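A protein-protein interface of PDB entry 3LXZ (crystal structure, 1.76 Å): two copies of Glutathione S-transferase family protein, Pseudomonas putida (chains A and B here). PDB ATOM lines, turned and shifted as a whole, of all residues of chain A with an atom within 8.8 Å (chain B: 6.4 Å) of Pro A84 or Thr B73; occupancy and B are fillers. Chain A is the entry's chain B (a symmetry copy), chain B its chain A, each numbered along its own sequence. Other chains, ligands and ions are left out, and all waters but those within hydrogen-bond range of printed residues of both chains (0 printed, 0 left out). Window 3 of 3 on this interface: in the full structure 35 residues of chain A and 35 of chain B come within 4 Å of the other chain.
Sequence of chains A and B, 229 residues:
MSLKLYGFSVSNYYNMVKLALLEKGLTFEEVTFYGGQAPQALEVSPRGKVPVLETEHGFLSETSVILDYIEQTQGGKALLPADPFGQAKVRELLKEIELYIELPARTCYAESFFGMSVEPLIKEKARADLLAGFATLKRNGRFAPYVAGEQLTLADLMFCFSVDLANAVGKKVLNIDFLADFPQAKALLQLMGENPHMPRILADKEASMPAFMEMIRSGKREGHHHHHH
Pro A84 touches just these residues of chain B: Tyr B69, Gln B72 and Thr B73.
Printed residues of chain A within 4 Å of Leu B60: Phe A85, Ala A88 and Lys A89.
Of the printed residues of chain A, Tyr B69 touches Pro A84, Phe A85 and Ala A88.
Thr B73 touches just one residue of chain A: Pro A84.
The nearest residue of chain A that does not touch Thr B73 is Phe A85 (5.4 Å).
Tyr B69 touches Pro A84 (CD1 to O, 3.8 Å).
Gln B72 touches Pro A84.
Pro A84 touches Thr B73 (CB to CG2, 3.6 Å).
CG of Leu B60 touches CE1 of Phe A85, at 3.5 Å.
Phe A85 touches Tyr B69.
CB of Ala A88 touches CD2 of Leu B60 (3.7 Å).
Tyr B69 touches Ala A88.
Leu B60 touches Lys A89.
No position is printed for both chains.
Of the 9 pairs that touch across the chains among the printed residues, none has its exchanged pair printed and touching as well.
Hydrophobic or aromatic side chains of chain A within 4 Å of the printed part of chain B: Pro A84, Phe A85 and Ala A88.
Of the 10 printed residues of chain B, 4 touch a printed residue of chain A.
Printed residues of chain B that touch a printed residue of chain A: Leu B60, Tyr B69, Gln B72 and Thr B73.
Hydrophobic or aromatic side chains of chain B that line the printed part of chain A: Leu B60 and Tyr B69.
Among the printed residues, 9 pairs touch across the chains.
Among the printed residues, no Asp or Glu carboxylate lies within 4 Å of a Lys or Arg side-chain nitrogen of the other chain.
The backbone carbonyl oxygen (O) of Tyr B69 sits at hydrogen-bond distance from the side-chain hydroxyl (OG1) of Thr B73.
OG1 of Thr B73 lies within hydrogen-bond range of NE2 of Gln B74 (3.0 Å).
The backbone carbonyl oxygen (O) of Pro A81 is in hydrogen-bond range of the side-chain amide nitrogen (NE2) of Gln A87 (3.0 Å).
OE1 of Gln A87 sits close to OE1 of Gln B72, 3.1 Å away.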
ATOM      1  N   LEU A  80     -32.959  10.383 -22.555  1.00  0.00           N
ATOM      2  CA  LEU A  80     -31.814   9.777 -21.858  1.00  0.00           C
ATOM      3  C   LEU A  80     -32.308   9.397 -20.478  1.00  0.00           C
ATOM      4  O   LEU A  80     -33.247  10.041 -19.987  1.00  0.00           O
ATOM      5  CB  LEU A  80     -30.721  10.823 -21.622  1.00  0.00           C
ATOM      6  CG  LEU A  80     -29.941  11.423 -22.773  1.00  0.00           C
ATOM      7  CD1 LEU A  80     -29.112  12.520 -22.148  1.00  0.00           C
ATOM      8  CD2 LEU A  80     -29.083  10.346 -23.380  1.00  0.00           C
ATOM      9  N   PRO A  81     -31.671   8.395 -19.835  1.00  0.00           N
ATOM     10  CA  PRO A  81     -31.977   8.084 -18.433  1.00  0.00           C
ATOM     11  C   PRO A  81     -31.474   9.185 -17.538  1.00  0.00           C
ATOM     12  O   PRO A  81     -30.734  10.030 -17.977  1.00  0.00           O
ATOM     13  CB  PRO A  81     -31.130   6.856 -18.133  1.00  0.00           C
ATOM     14  CG  PRO A  81     -30.061   6.848 -19.161  1.00  0.00           C
ATOM     15  CD  PRO A  81     -30.629   7.506 -20.387  1.00  0.00           C
ATOM     16  N   ALA A  82     -31.850   9.127 -16.268  1.00  0.00           N
ATOM     17  CA  ALA A  82     -31.518  10.208 -15.338  1.00  0.00           C
ATOM     18  C   ALA A  82     -30.078  10.107 -14.797  1.00  0.00           C
ATOM     19  O   ALA A  82     -29.525  11.103 -14.341  1.00  0.00           O
ATOM     20  CB  ALA A  82     -32.485  10.180 -14.204  1.00  0.00           C
ATOM     21  N   ASP A  83     -29.482   8.923 -14.828  1.00  0.00           N
ATOM     22  CA  ASP A  83     -28.215   8.668 -14.131  1.00  0.00           C
ATOM     23  C   ASP A  83     -27.025   8.878 -15.044  1.00  0.00           C
ATOM     24  O   ASP A  83     -27.076   8.504 -16.224  1.00  0.00           O
ATOM     25  CB  ASP A  83     -28.158   7.251 -13.525  1.00  0.00           C
ATOM     26  CG  ASP A  83     -28.270   6.147 -14.581  1.00  0.00           C
ATOM     27  OD1 ASP A  83     -29.360   6.029 -15.189  1.00  0.00           O
ATOM     28  OD2 ASP A  83     -27.292   5.364 -14.771  1.00  0.00           O
ATOM     29  N   PRO A  84     -25.923   9.411 -14.485  1.00  0.00           N
ATOM     30  CA  PRO A  84     -24.861   9.826 -15.358  1.00  0.00           C
ATOM     31  C   PRO A  84     -24.159   8.673 -16.043  1.00  0.00           C
ATOM     32  O   PRO A  84     -23.745   8.818 -17.199  1.00  0.00           O
ATOM     33  CB  PRO A  84     -23.889  10.571 -14.414  1.00  0.00           C
ATOM     34  CG  PRO A  84     -24.716  10.957 -13.253  1.00  0.00           C
ATOM     35  CD  PRO A  84     -25.673   9.828 -13.088  1.00  0.00           C
ATOM     36  N   PHE A  85     -23.994   7.542 -15.371  1.00  0.00           N
ATOM     37  CA  PHE A  85     -23.405   6.421 -16.077  1.00  0.00           C
ATOM     38  C   PHE A  85     -24.292   5.935 -17.228  1.00  0.00           C
ATOM     39  O   PHE A  85     -23.788   5.655 -18.344  1.00  0.00           O
ATOM     40  CB  PHE A  85     -23.062   5.251 -15.150  1.00  0.00           C
ATOM     41  CG  PHE A  85     -22.293   4.161 -15.846  1.00  0.00           C
ATOM     42  CD1 PHE A  85     -20.917   4.236 -15.964  1.00  0.00           C
ATOM     43  CD2 PHE A  85     -22.955   3.081 -16.421  1.00  0.00           C
ATOM     44  CE1 PHE A  85     -20.189   3.222 -16.604  1.00  0.00           C
ATOM     45  CE2 PHE A  85     -22.237   2.075 -17.088  1.00  0.00           C
ATOM     46  CZ  PHE A  85     -20.850   2.155 -17.177  1.00  0.00           C
ATOM     47  N   GLY A  86     -25.599   5.829 -16.968  1.00  0.00           N
ATOM     48  CA  GLY A  86     -26.563   5.406 -18.005  1.00  0.00           C
ATOM     49  C   GLY A  86     -26.550   6.346 -19.208  1.00  0.00           C
ATOM     50  O   GLY A  86     -26.653   5.903 -20.346  1.00  0.00           O
ATOM     51  N   GLN A  87     -26.412   7.640 -18.949  1.00  0.00           N
ATOM     52  CA  GLN A  87     -26.340   8.654 -20.033  1.00  0.00           C
ATOM     53  C   GLN A  87     -25.082   8.477 -20.885  1.00  0.00           C
ATOM     54  O   GLN A  87     -25.117   8.569 -22.113  1.00  0.00           O
ATOM     55  CB  GLN A  87     -26.357  10.077 -19.467  1.00  0.00           C
ATOM     56  CG  GLN A  87     -27.708  10.563 -19.000  1.00  0.00           C
ATOM     57  CD  GLN A  87     -27.650  11.850 -18.244  1.00  0.00           C
ATOM     58  OE1 GLN A  87     -26.589  12.449 -18.093  1.00  0.00           O
ATOM     59  NE2 GLN A  87     -28.806  12.306 -17.776  1.00  0.00           N
ATOM     60  N   ALA A  88     -23.960   8.247 -20.206  1.00  0.00           N
ATOM     61  CA  ALA A  88     -22.697   7.963 -20.868  1.00  0.00           C
ATOM     62  C   ALA A  88     -22.789   6.680 -21.702  1.00  0.00           C
ATOM     63  O   ALA A  88     -22.312   6.630 -22.834  1.00  0.00           O
ATOM     64  CB  ALA A  88     -21.566   7.909 -19.865  1.00  0.00           C
ATOM     65  N   LYS A  89     -23.439   5.648 -21.162  1.00  0.00           N
ATOM     66  CA  LYS A  89     -23.588   4.441 -21.944  1.00  0.00           C
ATOM     67  C   LYS A  89     -24.408   4.696 -23.223  1.00  0.00           C
ATOM     68  O   LYS A  89     -24.092   4.125 -24.267  1.00  0.00           O
ATOM     69  CB  LYS A  89     -24.197   3.320 -21.087  1.00  0.00           C
ATOM     70  CG  LYS A  89     -24.410   1.980 -21.785  1.00  0.00           C
ATOM     71  CD  LYS A  89     -23.177   1.365 -22.437  1.00  0.00           C
ATOM     72  CE  LYS A  89     -22.277   0.678 -21.459  1.00  0.00           C
ATOM     73  NZ  LYS A  89     -21.299  -0.161 -22.233  1.00  0.00           N
ATOM     74  N   VAL A  90     -25.452   5.523 -23.147  1.00  0.00           N
ATOM     75  CA  VAL A  90     -26.226   5.877 -24.342  1.00  0.00           C
ATOM     76  C   VAL A  90     -25.305   6.576 -25.336  1.00  0.00           C
ATOM     77  O   VAL A  90     -25.301   6.266 -26.519  1.00  0.00           O
ATOM     78  CB  VAL A  90     -27.436   6.786 -24.017  1.00  0.00           C
ATOM     79  CG1 VAL A  90     -28.080   7.409 -25.309  1.00  0.00           C
ATOM     80  CG2 VAL A  90     -28.506   6.012 -23.156  1.00  0.00           C
ATOM     81  N   ARG A  91     -24.497   7.521 -24.842  1.00  0.00           N
ATOM     82  CA  ARG A  91     -23.619   8.239 -25.751  1.00  0.00           C
ATOM     83  C   ARG A  91     -22.516   7.365 -26.362  1.00  0.00           C
ATOM     84  O   ARG A  91     -22.100   7.611 -27.486  1.00  0.00           O
ATOM     85  CB  ARG A  91     -23.064   9.472 -25.036  1.00  0.00           C
ATOM     86  CG  ARG A  91     -24.163  10.521 -24.818  1.00  0.00           C
ATOM     87  CD  ARG A  91     -23.813  11.511 -23.703  1.00  0.00           C
ATOM     88  NE  ARG A  91     -24.774  12.613 -23.702  1.00  0.00           N
ATOM     89  CZ  ARG A  91     -25.227  13.206 -22.594  1.00  0.00           C
ATOM     90  NH1 ARG A  91     -24.840  12.763 -21.402  1.00  0.00           N
ATOM     91  NH2 ARG A  91     -26.109  14.194 -22.689  1.00  0.00           N
ATOM     92  N   LEU B   3     -11.261   5.107  -9.673  1.00  0.00           N
ATOM     93  CA  LEU B   3     -11.242   5.076 -11.148  1.00  0.00           C
ATOM     94  C   LEU B   3      -9.984   4.409 -11.675  1.00  0.00           C
ATOM     95  O   LEU B   3      -8.871   4.645 -11.158  1.00  0.00           O
ATOM     96  CB  LEU B   3     -11.321   6.485 -11.743  1.00  0.00           C
ATOM     97  CG  LEU B   3     -12.562   7.328 -11.480  1.00  0.00           C
ATOM     98  CD1 LEU B   3     -12.335   8.684 -12.126  1.00  0.00           C
ATOM     99  CD2 LEU B   3     -13.818   6.671 -12.018  1.00  0.00           C
ATOM    100  N   LEU B  60     -16.535   2.292 -19.477  1.00  0.00           N
ATOM    101  CA  LEU B  60     -16.915   3.226 -20.559  1.00  0.00           C
ATOM    102  C   LEU B  60     -15.740   3.369 -21.499  1.00  0.00           C
ATOM    103  O   LEU B  60     -14.620   3.596 -21.026  1.00  0.00           O
ATOM    104  CB  LEU B  60     -17.244   4.622 -20.002  1.00  0.00           C
ATOM    105  CG  LEU B  60     -18.530   4.875 -19.235  1.00  0.00           C
ATOM    106  CD1 LEU B  60     -18.517   6.227 -18.555  1.00  0.00           C
ATOM    107  CD2 LEU B  60     -19.756   4.745 -20.161  1.00  0.00           C
ATOM    108  N   ASP B  68     -16.765  13.405 -20.943  1.00  0.00           N
ATOM    109  CA  ASP B  68     -18.056  13.939 -20.546  1.00  0.00           C
ATOM    110  C   ASP B  68     -18.538  13.356 -19.219  1.00  0.00           C
ATOM    111  O   ASP B  68     -19.054  14.112 -18.376  1.00  0.00           O
ATOM    112  CB  ASP B  68     -19.116  13.678 -21.619  1.00  0.00           C
ATOM    113  CG  ASP B  68     -19.133  14.732 -22.720  1.00  0.00           C
ATOM    114  OD1 ASP B  68     -18.513  15.827 -22.586  1.00  0.00           O
ATOM    115  OD2 ASP B  68     -19.796  14.439 -23.743  1.00  0.00           O
ATOM    116  N   TYR B  69     -18.374  12.042 -19.045  1.00  0.00           N
ATOM    117  CA  TYR B  69     -18.667  11.366 -17.782  1.00  0.00           C
ATOM    118  C   TYR B  69     -17.829  11.943 -16.656  1.00  0.00           C
ATOM    119  O   TYR B  69     -18.368  12.234 -15.607  1.00  0.00           O
ATOM    120  CB  TYR B  69     -18.408   9.868 -17.892  1.00  0.00           C
ATOM    121  CG  TYR B  69     -18.721   9.111 -16.622  1.00  0.00           C
ATOM    122  CD1 TYR B  69     -20.021   8.769 -16.280  1.00  0.00           C
ATOM    123  CD2 TYR B  69     -17.697   8.725 -15.766  1.00  0.00           C
ATOM    124  CE1 TYR B  69     -20.295   8.048 -15.098  1.00  0.00           C
ATOM    125  CE2 TYR B  69     -17.959   8.019 -14.586  1.00  0.00           C
ATOM    126  CZ  TYR B  69     -19.266   7.685 -14.271  1.00  0.00           C
ATOM    127  OH  TYR B  69     -19.519   6.978 -13.120  1.00  0.00           O
ATOM    128  N   ILE B  70     -16.531  12.143 -16.893  1.00  0.00           N
ATOM    129  CA  ILE B  70     -15.667  12.730 -15.864  1.00  0.00           C
ATOM    130  C   ILE B  70     -16.129  14.128 -15.430  1.00  0.00           C
ATOM    131  O   ILE B  70     -16.209  14.411 -14.220  1.00  0.00           O
ATOM    132  CB  ILE B  70     -14.189  12.690 -16.273  1.00  0.00           C
ATOM    133  CG1 ILE B  70     -13.679  11.261 -16.300  1.00  0.00           C
ATOM    134  CG2 ILE B  70     -13.299  13.459 -15.275  1.00  0.00           C
ATOM    135  CD1 ILE B  70     -12.290  11.125 -16.958  1.00  0.00           C
ATOM    136  N   GLU B  71     -16.437  15.004 -16.393  1.00  0.00           N
ATOM    137  CA  GLU B  71     -16.957  16.345 -16.077  1.00  0.00           C
ATOM    138  C   GLU B  71     -18.186  16.347 -15.148  1.00  0.00           C
ATOM    139  O   GLU B  71     -18.259  17.098 -14.174  1.00  0.00           O
ATOM    140  CB  GLU B  71     -17.288  17.130 -17.349  1.00  0.00           C
ATOM    141  CG  GLU B  71     -16.121  17.844 -17.996  1.00  0.00           C
ATOM    142  CD  GLU B  71     -15.185  18.538 -16.987  1.00  0.00           C
ATOM    143  OE1 GLU B  71     -14.106  17.967 -16.783  1.00  0.00           O
ATOM    144  OE2 GLU B  71     -15.533  19.605 -16.391  1.00  0.00           O
ATOM    145  N   GLN B  72     -19.138  15.485 -15.504  1.00  0.00           N
ATOM    146  CA  GLN B  72     -20.408  15.331 -14.866  1.00  0.00           C
ATOM    147  C   GLN B  72     -20.298  14.793 -13.442  1.00  0.00           C
ATOM    148  O   GLN B  72     -21.028  15.239 -12.559  1.00  0.00           O
ATOM    149  CB  GLN B  72     -21.181  14.308 -15.692  1.00  0.00           C
ATOM    150  CG  GLN B  72     -22.493  13.948 -15.139  1.00  0.00           C
ATOM    151  CD  GLN B  72     -23.544  14.583 -15.935  1.00  0.00           C
ATOM    152  OE1 GLN B  72     -24.217  13.916 -16.748  1.00  0.00           O
ATOM    153  NE2 GLN B  72     -23.663  15.917 -15.788  1.00  0.00           N
ATOM    154  N   THR B  73     -19.398  13.841 -13.228  1.00  0.00           N
ATOM    155  CA  THR B  73     -19.405  13.058 -11.996  1.00  0.00           C
ATOM    156  C   THR B  73     -18.299  13.420 -11.012  1.00  0.00           C
ATOM    157  O   THR B  73     -18.406  13.114  -9.823  1.00  0.00           O
ATOM    158  CB  THR B  73     -19.367  11.536 -12.254  1.00  0.00           C
ATOM    159  OG1 THR B  73     -18.165  11.166 -12.957  1.00  0.00           O
ATOM    160  CG2 THR B  73     -20.626  11.088 -13.029  1.00  0.00           C
ATOM    161  N   GLN B  74     -17.256  14.093 -11.485  1.00  0.00           N
ATOM    162  CA  GLN B  74     -16.060  14.242 -10.656  1.00  0.00           C
ATOM    163  C   GLN B  74     -15.848  15.670 -10.241  1.00  0.00           C
ATOM    164  O   GLN B  74     -16.229  16.590 -10.979  1.00  0.00           O
ATOM    165  CB  GLN B  74     -14.794  13.733 -11.367  1.00  0.00           C
ATOM    166  CG  GLN B  74     -14.865  12.276 -11.902  1.00  0.00           C
ATOM    167  CD  GLN B  74     -15.059  11.230 -10.804  1.00  0.00           C
ATOM    168  OE1 GLN B  74     -14.297  11.188  -9.831  1.00  0.00           O
ATOM    169  NE2 GLN B  74     -16.079  10.373 -10.965  1.00  0.00           N
ATOM    170  N   GLY B  75     -15.184  15.835  -9.091  1.00  0.00           N
ATOM    171  CA  GLY B  75     -14.700  17.146  -8.590  1.00  0.00           C
ATOM    172  C   GLY B  75     -13.510  17.712  -9.344  1.00  0.00           C
ATOM    173  O   GLY B  75     -13.057  17.133 -10.338  1.00  0.00           O
